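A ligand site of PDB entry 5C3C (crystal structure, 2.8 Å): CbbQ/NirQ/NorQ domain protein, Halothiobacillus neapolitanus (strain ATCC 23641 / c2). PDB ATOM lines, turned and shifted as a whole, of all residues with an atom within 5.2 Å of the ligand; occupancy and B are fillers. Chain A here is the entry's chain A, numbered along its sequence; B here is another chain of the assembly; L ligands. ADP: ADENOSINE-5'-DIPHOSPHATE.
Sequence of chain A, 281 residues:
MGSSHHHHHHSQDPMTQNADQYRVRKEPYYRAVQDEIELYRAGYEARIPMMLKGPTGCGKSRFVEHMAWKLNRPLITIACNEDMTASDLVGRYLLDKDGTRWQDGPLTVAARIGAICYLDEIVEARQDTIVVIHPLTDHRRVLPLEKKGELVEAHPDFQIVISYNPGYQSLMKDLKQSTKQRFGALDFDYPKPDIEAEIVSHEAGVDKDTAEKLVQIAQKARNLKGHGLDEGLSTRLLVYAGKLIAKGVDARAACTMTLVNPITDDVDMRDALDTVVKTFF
OG of Ser 61 sits at hydrogen-bond distance from OH of Tyr 118, at 3.1 Å. The side-chain hydroxyl of Ser 61 lies within hydrogen-bond range of the side-chain carboxylate of Asp 120, at 2.9 Å. The backbone NH (N) of Arg 236 sits close to the side-chain hydroxyl (OG) of Ser 234. The backbone carbonyl oxygen of Gly 57 lies within hydrogen-bond range of the side-chain hydroxyl of Thr 235, 3.0 Å away. The side-chain carboxylate of Glu 203 lies within salt-bridge range of the guanidinium group of Arg 62, 3.0 Å away. SG of Cys 58 lies within hydrogen-bond range of O of Pro 55 (3.4 Å).
A nitrogen (N6) of the ligand sits at hydrogen-bond distance from the backbone carbonyl oxygen (O) of Arg 31 (2.5 Å). An oxygen (O2B) of the ligand sits at hydrogen-bond distance from the backbone NH of Lys 60, at 3.2 Å. An oxygen (O2B) of the ligand lies within salt-bridge range of the side-chain amino group (NZ) of Lys 60. An oxygen (O1B) of the ligand is in hydrogen-bond range of the backbone NH (N) of Ser 61 (2.7 Å). The side-chain hydroxyl (OG) of Ser 61 sits at hydrogen-bond distance from an oxygen (O1B) of the ligand (2.6 Å). The guanidinium group (NH2) of Arg 236 is in salt-bridge range of an oxygen (O2A) of the ligand, at 2.8 Å. The backbone NH (N) of Gly 57 lies within hydrogen-bond range of an oxygen (O3B) of the ligand (2.8 Å). The backbone NH (N) of Gly 59 sits at hydrogen-bond distance from an oxygen (O3A) of the ligand, 3.0 Å away. N of Arg 62 sits at hydrogen-bond distance from O1A of the ligand, at 3.2 Å. An oxygen (O2') of the ligand lies within hydrogen-bond range of the guanidinium group (NH1) of Arg 62 (3.1 Å). The side-chain carboxylate (OE1) of Glu 203 lies within hydrogen-bond range of an oxygen (O2') of the ligand (3.1 Å). O2B of the ligand sits at hydrogen-bond distance from N of Cys 58, at 3.2 Å.
The backbone carbonyl oxygen (O) of Tyr 29 sits close to a nitrogen (N7) of the ligand, at 3.4 Å. Tyr 30 touches the ligand (CE1 to N6, 3.3 Å). Pro 55 touches the ligand (O to O2B, 3.8 Å). Thr 56 touches the ligand (C to O3B, 3.997 Å). Ile 199 touches the ligand. CG2 of Thr 235 touches N3 of the ligand, at 3.998 Å. Hydrophobic or aromatic side chains that line the ligand: Tyr 30 and Ile 199. Within 4 Å of the ligand: Tyr 29, Tyr 30, Arg 31, Pro 55, Thr 56, Gly 57, Cys 58, Gly 59, Lys 60, Ser 61, Arg 62, Ile 199, Glu 203, Thr 235 and Arg 236. Along chain A the residues within 4 Å of the ligand span positions 29 to 236.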
ATOM      1  N   TYR A  29      30.233  23.721 -13.863  1.00  0.00           N
ATOM      2  CA  TYR A  29      31.225  23.602 -12.804  1.00  0.00           C
ATOM      3  C   TYR A  29      30.591  23.360 -11.445  1.00  0.00           C
ATOM      4  O   TYR A  29      30.036  24.285 -10.848  1.00  0.00           O
ATOM      5  CB  TYR A  29      32.106  24.863 -12.760  1.00  0.00           C
ATOM      6  CG  TYR A  29      32.975  24.965 -11.524  1.00  0.00           C
ATOM      7  CD1 TYR A  29      34.130  24.204 -11.408  1.00  0.00           C
ATOM      8  CD2 TYR A  29      32.649  25.832 -10.491  1.00  0.00           C
ATOM      9  CE1 TYR A  29      34.936  24.305 -10.286  1.00  0.00           C
ATOM     10  CE2 TYR A  29      33.444  25.933  -9.369  1.00  0.00           C
ATOM     11  CZ  TYR A  29      34.588  25.168  -9.271  1.00  0.00           C
ATOM     12  OH  TYR A  29      35.383  25.268  -8.149  1.00  0.00           O
ATOM     13  N   TYR A  30      30.675  22.131 -10.944  1.00  0.00           N
ATOM     14  CA  TYR A  30      30.200  21.840  -9.603  1.00  0.00           C
ATOM     15  C   TYR A  30      31.296  21.233  -8.732  1.00  0.00           C
ATOM     16  O   TYR A  30      31.872  20.204  -9.057  1.00  0.00           O
ATOM     17  CB  TYR A  30      28.987  20.908  -9.630  1.00  0.00           C
ATOM     18  CG  TYR A  30      28.436  20.621  -8.251  1.00  0.00           C
ATOM     19  CD1 TYR A  30      27.582  21.513  -7.626  1.00  0.00           C
ATOM     20  CD2 TYR A  30      28.800  19.463  -7.568  1.00  0.00           C
ATOM     21  CE1 TYR A  30      27.088  21.268  -6.363  1.00  0.00           C
ATOM     22  CE2 TYR A  30      28.307  19.208  -6.304  1.00  0.00           C
ATOM     23  CZ  TYR A  30      27.450  20.116  -5.702  1.00  0.00           C
ATOM     24  OH  TYR A  30      26.965  19.869  -4.449  1.00  0.00           O
ATOM     25  N   ARG A  31      31.564  21.897  -7.614  1.00  0.00           N
ATOM     26  CA  ARG A  31      32.558  21.425  -6.654  1.00  0.00           C
ATOM     27  C   ARG A  31      31.872  20.642  -5.528  1.00  0.00           C
ATOM     28  O   ARG A  31      31.053  21.179  -4.791  1.00  0.00           O
ATOM     29  CB  ARG A  31      33.345  22.605  -6.085  1.00  0.00           C
ATOM     30  CG  ARG A  31      33.987  22.365  -4.741  1.00  0.00           C
ATOM     31  CD  ARG A  31      35.232  21.490  -4.819  1.00  0.00           C
ATOM     32  NE  ARG A  31      35.791  21.254  -3.497  1.00  0.00           N
ATOM     33  CZ  ARG A  31      36.958  20.677  -3.263  1.00  0.00           C
ATOM     34  NH1 ARG A  31      37.716  20.263  -4.271  1.00  0.00           N
ATOM     35  NH2 ARG A  31      37.387  20.504  -2.020  1.00  0.00           N
ATOM     36  N   ALA A  32      32.214  19.359  -5.424  1.00  0.00           N
ATOM     37  CA  ALA A  32      31.585  18.484  -4.430  1.00  0.00           C
ATOM     38  C   ALA A  32      32.008  18.849  -3.020  1.00  0.00           C
ATOM     39  O   ALA A  32      33.198  18.936  -2.714  1.00  0.00           O
ATOM     40  CB  ALA A  32      31.926  17.038  -4.726  1.00  0.00           C
ATOM     41  N   VAL A  33      31.025  19.068  -2.156  1.00  0.00           N
ATOM     42  CA  VAL A  33      31.285  19.396  -0.762  1.00  0.00           C
ATOM     43  C   VAL A  33      31.455  18.114   0.056  1.00  0.00           C
ATOM     44  O   VAL A  33      32.342  18.014   0.898  1.00  0.00           O
ATOM     45  CB  VAL A  33      30.167  20.255  -0.164  1.00  0.00           C
ATOM     46  CG1 VAL A  33      30.530  20.701   1.250  1.00  0.00           C
ATOM     47  CG2 VAL A  33      29.900  21.462  -1.049  1.00  0.00           C
ATOM     48  N   PRO A  55      19.635  26.249   1.815  1.00  0.00           N
ATOM     49  CA  PRO A  55      19.414  27.695   1.638  1.00  0.00           C
ATOM     50  C   PRO A  55      19.542  28.128   0.175  1.00  0.00           C
ATOM     51  O   PRO A  55      19.898  27.305  -0.674  1.00  0.00           O
ATOM     52  CB  PRO A  55      20.518  28.334   2.486  1.00  0.00           C
ATOM     53  CG  PRO A  55      20.979  27.252   3.410  1.00  0.00           C
ATOM     54  CD  PRO A  55      20.815  25.973   2.648  1.00  0.00           C
ATOM     55  N   THR A  56      19.251  29.391  -0.105  1.00  0.00           N
ATOM     56  CA  THR A  56      19.350  29.903  -1.465  1.00  0.00           C
ATOM     57  C   THR A  56      20.810  30.017  -1.899  1.00  0.00           C
ATOM     58  O   THR A  56      21.655  30.481  -1.135  1.00  0.00           O
ATOM     59  CB  THR A  56      18.680  31.281  -1.613  1.00  0.00           C
ATOM     60  OG1 THR A  56      19.444  32.272  -0.905  1.00  0.00           O
ATOM     61  CG2 THR A  56      17.261  31.249  -1.066  1.00  0.00           C
ATOM     62  N   GLY A  57      21.081  29.601  -3.131  1.00  0.00           N
ATOM     63  CA  GLY A  57      22.417  29.719  -3.695  1.00  0.00           C
ATOM     64  C   GLY A  57      23.466  28.887  -2.992  1.00  0.00           C
ATOM     65  O   GLY A  57      24.552  29.387  -2.689  1.00  0.00           O
ATOM     66  N   CYS A  58      23.153  27.627  -2.719  1.00  0.00           N
ATOM     67  CA  CYS A  58      24.147  26.707  -2.159  1.00  0.00           C
ATOM     68  C   CYS A  58      24.505  25.638  -3.188  1.00  0.00           C
ATOM     69  O   CYS A  58      25.083  24.607  -2.849  1.00  0.00           O
ATOM     70  CB  CYS A  58      23.639  26.071  -0.864  1.00  0.00           C
ATOM     71  SG  CYS A  58      22.248  24.942  -1.060  1.00  0.00           S
ATOM     72  N   GLY A  59      24.144  25.902  -4.444  1.00  0.00           N
ATOM     73  CA  GLY A  59      24.535  25.036  -5.535  1.00  0.00           C
ATOM     74  C   GLY A  59      23.586  23.891  -5.828  1.00  0.00           C
ATOM     75  O   GLY A  59      23.982  22.883  -6.413  1.00  0.00           O
ATOM     76  N   LYS A  60      22.319  24.048  -5.443  1.00  0.00           N
ATOM     77  CA  LYS A  60      21.316  23.005  -5.667  1.00  0.00           C
ATOM     78  C   LYS A  60      20.974  22.863  -7.148  1.00  0.00           C
ATOM     79  O   LYS A  60      21.003  21.760  -7.696  1.00  0.00           O
ATOM     80  CB  LYS A  60      20.052  23.295  -4.878  1.00  0.00           C
ATOM     81  CG  LYS A  60      20.168  23.027  -3.380  1.00  0.00           C
ATOM     82  CD  LYS A  60      18.847  23.254  -2.655  1.00  0.00           C
ATOM     83  CE  LYS A  60      18.656  24.718  -2.277  1.00  0.00           C
ATOM     84  NZ  LYS A  60      18.392  25.612  -3.434  1.00  0.00           N
ATOM     85  N   SER A  61      20.654  23.978  -7.796  1.00  0.00           N
ATOM     86  CA  SER A  61      20.309  23.960  -9.207  1.00  0.00           C
ATOM     87  C   SER A  61      21.478  23.486 -10.044  1.00  0.00           C
ATOM     88  O   SER A  61      21.314  22.689 -10.955  1.00  0.00           O
ATOM     89  CB  SER A  61      19.854  25.346  -9.686  1.00  0.00           C
ATOM     90  OG  SER A  61      18.667  25.750  -9.008  1.00  0.00           O
ATOM     91  N   ARG A  62      22.667  23.983  -9.721  1.00  0.00           N
ATOM     92  CA  ARG A  62      23.879  23.603 -10.437  1.00  0.00           C
ATOM     93  C   ARG A  62      24.176  22.111 -10.300  1.00  0.00           C
ATOM     94  O   ARG A  62      24.609  21.463 -11.261  1.00  0.00           O
ATOM     95  CB  ARG A  62      25.074  24.426  -9.939  1.00  0.00           C
ATOM     96  CG  ARG A  62      26.394  24.061 -10.587  1.00  0.00           C
ATOM     97  CD  ARG A  62      27.143  25.305 -11.017  1.00  0.00           C
ATOM     98  NE  ARG A  62      26.528  25.934 -12.179  1.00  0.00           N
ATOM     99  CZ  ARG A  62      26.980  27.042 -12.757  1.00  0.00           C
ATOM    100  NH1 ARG A  62      28.055  27.647 -12.267  1.00  0.00           N
ATOM    101  NH2 ARG A  62      26.357  27.548 -13.814  1.00  0.00           N
ATOM    102  N   TYR A 118      13.292  19.074 -13.081  1.00  0.00           N
ATOM    103  CA  TYR A 118      13.719  19.777 -11.885  1.00  0.00           C
ATOM    104  C   TYR A 118      12.739  20.868 -11.487  1.00  0.00           C
ATOM    105  O   TYR A 118      12.672  21.922 -12.121  1.00  0.00           O
ATOM    106  CB  TYR A 118      15.121  20.357 -12.091  1.00  0.00           C
ATOM    107  CG  TYR A 118      15.666  21.140 -10.922  1.00  0.00           C
ATOM    108  CD1 TYR A 118      16.200  22.413 -11.099  1.00  0.00           C
ATOM    109  CD2 TYR A 118      15.660  20.619  -9.631  1.00  0.00           C
ATOM    110  CE1 TYR A 118      16.713  23.135 -10.039  1.00  0.00           C
ATOM    111  CE2 TYR A 118      16.163  21.340  -8.569  1.00  0.00           C
ATOM    112  CZ  TYR A 118      16.684  22.599  -8.773  1.00  0.00           C
ATOM    113  OH  TYR A 118      17.186  23.319  -7.721  1.00  0.00           O
ATOM    114  N   ASP A 120      12.218  23.565  -9.345  1.00  0.00           N
ATOM    115  CA  ASP A 120      12.911  24.493  -8.465  1.00  0.00           C
ATOM    116  C   ASP A 120      11.897  25.302  -7.654  1.00  0.00           C
ATOM    117  O   ASP A 120      10.834  25.651  -8.154  1.00  0.00           O
ATOM    118  CB  ASP A 120      13.822  25.420  -9.273  1.00  0.00           C
ATOM    119  CG  ASP A 120      14.896  26.078  -8.425  1.00  0.00           C
ATOM    120  OD1 ASP A 120      14.719  26.153  -7.183  1.00  0.00           O
ATOM    121  OD2 ASP A 120      15.917  26.512  -8.993  1.00  0.00           O
ATOM    122  N   PRO A 191      29.012  25.435   1.585  1.00  0.00           N
ATOM    123  CA  PRO A 191      30.217  24.620   1.787  1.00  0.00           C
ATOM    124  C   PRO A 191      31.190  25.186   2.816  1.00  0.00           C
ATOM    125  O   PRO A 191      31.076  26.344   3.231  1.00  0.00           O
ATOM    126  CB  PRO A 191      30.870  24.603   0.401  1.00  0.00           C
ATOM    127  CG  PRO A 191      30.279  25.757  -0.328  1.00  0.00           C
ATOM    128  CD  PRO A 191      28.885  25.871   0.180  1.00  0.00           C
ATOM    129  N   ILE A 199      35.399  28.012  -4.970  1.00  0.00           N
ATOM    130  CA  ILE A 199      34.271  28.204  -5.885  1.00  0.00           C
ATOM    131  C   ILE A 199      34.196  29.647  -6.384  1.00  0.00           C
ATOM    132  O   ILE A 199      33.973  29.897  -7.571  1.00  0.00           O
ATOM    133  CB  ILE A 199      32.938  27.819  -5.221  1.00  0.00           C
ATOM    134  CG1 ILE A 199      32.982  26.373  -4.738  1.00  0.00           C
ATOM    135  CG2 ILE A 199      31.785  28.032  -6.188  1.00  0.00           C
ATOM    136  CD1 ILE A 199      31.858  25.990  -3.811  1.00  0.00           C
ATOM    137  N   GLU A 203      34.724  30.963 -10.299  1.00  0.00           N
ATOM    138  CA  GLU A 203      33.603  31.544 -11.029  1.00  0.00           C
ATOM    139  C   GLU A 203      33.739  33.044 -11.245  1.00  0.00           C
ATOM    140  O   GLU A 203      33.485  33.542 -12.341  1.00  0.00           O
ATOM    141  CB  GLU A 203      32.297  31.243 -10.302  1.00  0.00           C
ATOM    142  CG  GLU A 203      31.956  29.756 -10.210  1.00  0.00           C
ATOM    143  CD  GLU A 203      31.771  29.120 -11.577  1.00  0.00           C
ATOM    144  OE1 GLU A 203      30.629  29.110 -12.085  1.00  0.00           O
ATOM    145  OE2 GLU A 203      32.769  28.629 -12.147  1.00  0.00           O
ATOM    146  N   SER A 234      23.236  33.989  -0.512  1.00  0.00           N
ATOM    147  CA  SER A 234      23.619  33.174  -1.662  1.00  0.00           C
ATOM    148  C   SER A 234      25.114  33.250  -1.971  1.00  0.00           C
ATOM    149  O   SER A 234      25.722  34.323  -1.863  1.00  0.00           O
ATOM    150  CB  SER A 234      22.818  33.582  -2.897  1.00  0.00           C
ATOM    151  OG  SER A 234      23.182  32.819  -4.034  1.00  0.00           O
ATOM    152  N   THR A 235      25.694  32.119  -2.359  1.00  0.00           N
ATOM    153  CA  THR A 235      27.074  32.077  -2.807  1.00  0.00           C
ATOM    154  C   THR A 235      27.240  32.910  -4.080  1.00  0.00           C
ATOM    155  O   THR A 235      28.315  33.462  -4.337  1.00  0.00           O
ATOM    156  CB  THR A 235      27.529  30.609  -3.069  1.00  0.00           C
ATOM    157  OG1 THR A 235      27.374  29.834  -1.869  1.00  0.00           O
ATOM    158  CG2 THR A 235      28.991  30.560  -3.505  1.00  0.00           C
ATOM    159  N   ARG A 236      26.178  33.006  -4.862  1.00  0.00           N
ATOM    160  CA  ARG A 236      26.189  33.793  -6.090  1.00  0.00           C
ATOM    161  C   ARG A 236      26.507  35.259  -5.839  1.00  0.00           C
ATOM    162  O   ARG A 236      27.127  35.931  -6.661  1.00  0.00           O
ATOM    163  CB  ARG A 236      24.853  33.666  -6.822  1.00  0.00           C
ATOM    164  CG  ARG A 236      24.712  34.540  -8.049  1.00  0.00           C
ATOM    165  CD  ARG A 236      24.101  33.753  -9.179  1.00  0.00           C
ATOM    166  NE  ARG A 236      22.898  33.069  -8.730  1.00  0.00           N
ATOM    167  CZ  ARG A 236      22.188  32.244  -9.485  1.00  0.00           C
ATOM    168  NH1 ARG A 236      22.545  32.029 -10.742  1.00  0.00           N
ATOM    169  NH2 ARG A 236      21.111  31.655  -8.976  1.00  0.00           N
ATOM    170  N   VAL A 239      30.139  35.570  -5.725  1.00  0.00           N
ATOM    171  CA  VAL A 239      30.654  35.513  -7.089  1.00  0.00           C
ATOM    172  C   VAL A 239      30.511  36.873  -7.760  1.00  0.00           C
ATOM    173  O   VAL A 239      31.415  37.319  -8.470  1.00  0.00           O
ATOM    174  CB  VAL A 239      29.918  34.440  -7.918  1.00  0.00           C
ATOM    175  CG1 VAL A 239      30.352  34.496  -9.375  1.00  0.00           C
ATOM    176  CG2 VAL A 239      30.183  33.057  -7.338  1.00  0.00           C
ATOM    177  N   ARG B 182      19.677  37.369  -6.701  1.00  0.00           N
ATOM    178  CA  ARG B 182      20.143  37.137  -8.069  1.00  0.00           C
ATOM    179  C   ARG B 182      20.608  38.450  -8.695  1.00  0.00           C
ATOM    180  O   ARG B 182      21.004  38.476  -9.857  1.00  0.00           O
ATOM    181  CB  ARG B 182      19.039  36.508  -8.919  1.00  0.00           C
ATOM    182  CG  ARG B 182      18.682  35.097  -8.511  1.00  0.00           C
ATOM    183  CD  ARG B 182      17.520  34.544  -9.328  1.00  0.00           C
ATOM    184  NE  ARG B 182      17.156  33.200  -8.891  1.00  0.00           N
ATOM    185  CZ  ARG B 182      17.651  32.075  -9.404  1.00  0.00           C
ATOM    186  NH1 ARG B 182      18.515  32.140 -10.419  1.00  0.00           N
ATOM    187  NH2 ARG B 182      17.278  30.898  -8.935  1.00  0.00           N
HETATM  188  PB  ADP L   1      20.570  27.211  -5.676  1.00  0.00           P
HETATM  189  O1B ADP L   1      19.959  26.423  -6.806  1.00  0.00           O
HETATM  190  O2B ADP L   1      20.619  26.473  -4.352  1.00  0.00           O
HETATM  191  O3B ADP L   1      20.077  28.628  -5.574  1.00  0.00           O
HETATM  192  PA  ADP L   1      22.569  28.008  -7.488  1.00  0.00           P
HETATM  193  O1A ADP L   1      22.529  26.959  -8.571  1.00  0.00           O
HETATM  194  O2A ADP L   1      21.818  29.301  -7.643  1.00  0.00           O
HETATM  195  O3A ADP L   1      22.123  27.331  -6.091  1.00  0.00           O
HETATM  196  O5' ADP L   1      24.107  28.377  -7.190  1.00  0.00           O
HETATM  197  C5' ADP L   1      24.515  29.741  -7.237  1.00  0.00           C
HETATM  198  C4' ADP L   1      25.996  29.842  -7.579  1.00  0.00           C
HETATM  199  O4' ADP L   1      26.770  28.912  -6.818  1.00  0.00           O
HETATM  200  C3' ADP L   1      26.251  29.507  -9.038  1.00  0.00           C
HETATM  201  O3' ADP L   1      26.411  30.717  -9.796  1.00  0.00           O
HETATM  202  C2' ADP L   1      27.543  28.706  -9.052  1.00  0.00           C
HETATM  203  O2' ADP L   1      28.547  29.429  -9.762  1.00  0.00           O
HETATM  204  C1' ADP L   1      27.925  28.560  -7.595  1.00  0.00           C
HETATM  205  N9  ADP L   1      28.398  27.180  -7.313  1.00  0.00           N
HETATM  206  C8  ADP L   1      28.929  26.341  -8.220  1.00  0.00           C
HETATM  207  N7  ADP L   1      29.293  25.163  -7.646  1.00  0.00           N
HETATM  208  C5  ADP L   1      28.993  25.248  -6.331  1.00  0.00           C
HETATM  209  C6  ADP L   1      29.108  24.353  -5.159  1.00  0.00           C
HETATM  210  N6  ADP L   1      29.628  23.118  -5.266  1.00  0.00           N
HETATM  211  N1  ADP L   1      28.681  24.840  -3.964  1.00  0.00           N
HETATM  212  C2  ADP L   1      28.163  26.068  -3.835  1.00  0.00           C
HETATM  213  N3  ADP L   1      28.024  26.927  -4.866  1.00  0.00           N
HETATM  214  C4  ADP L   1      28.413  26.582  -6.112  1.00  0.00           C
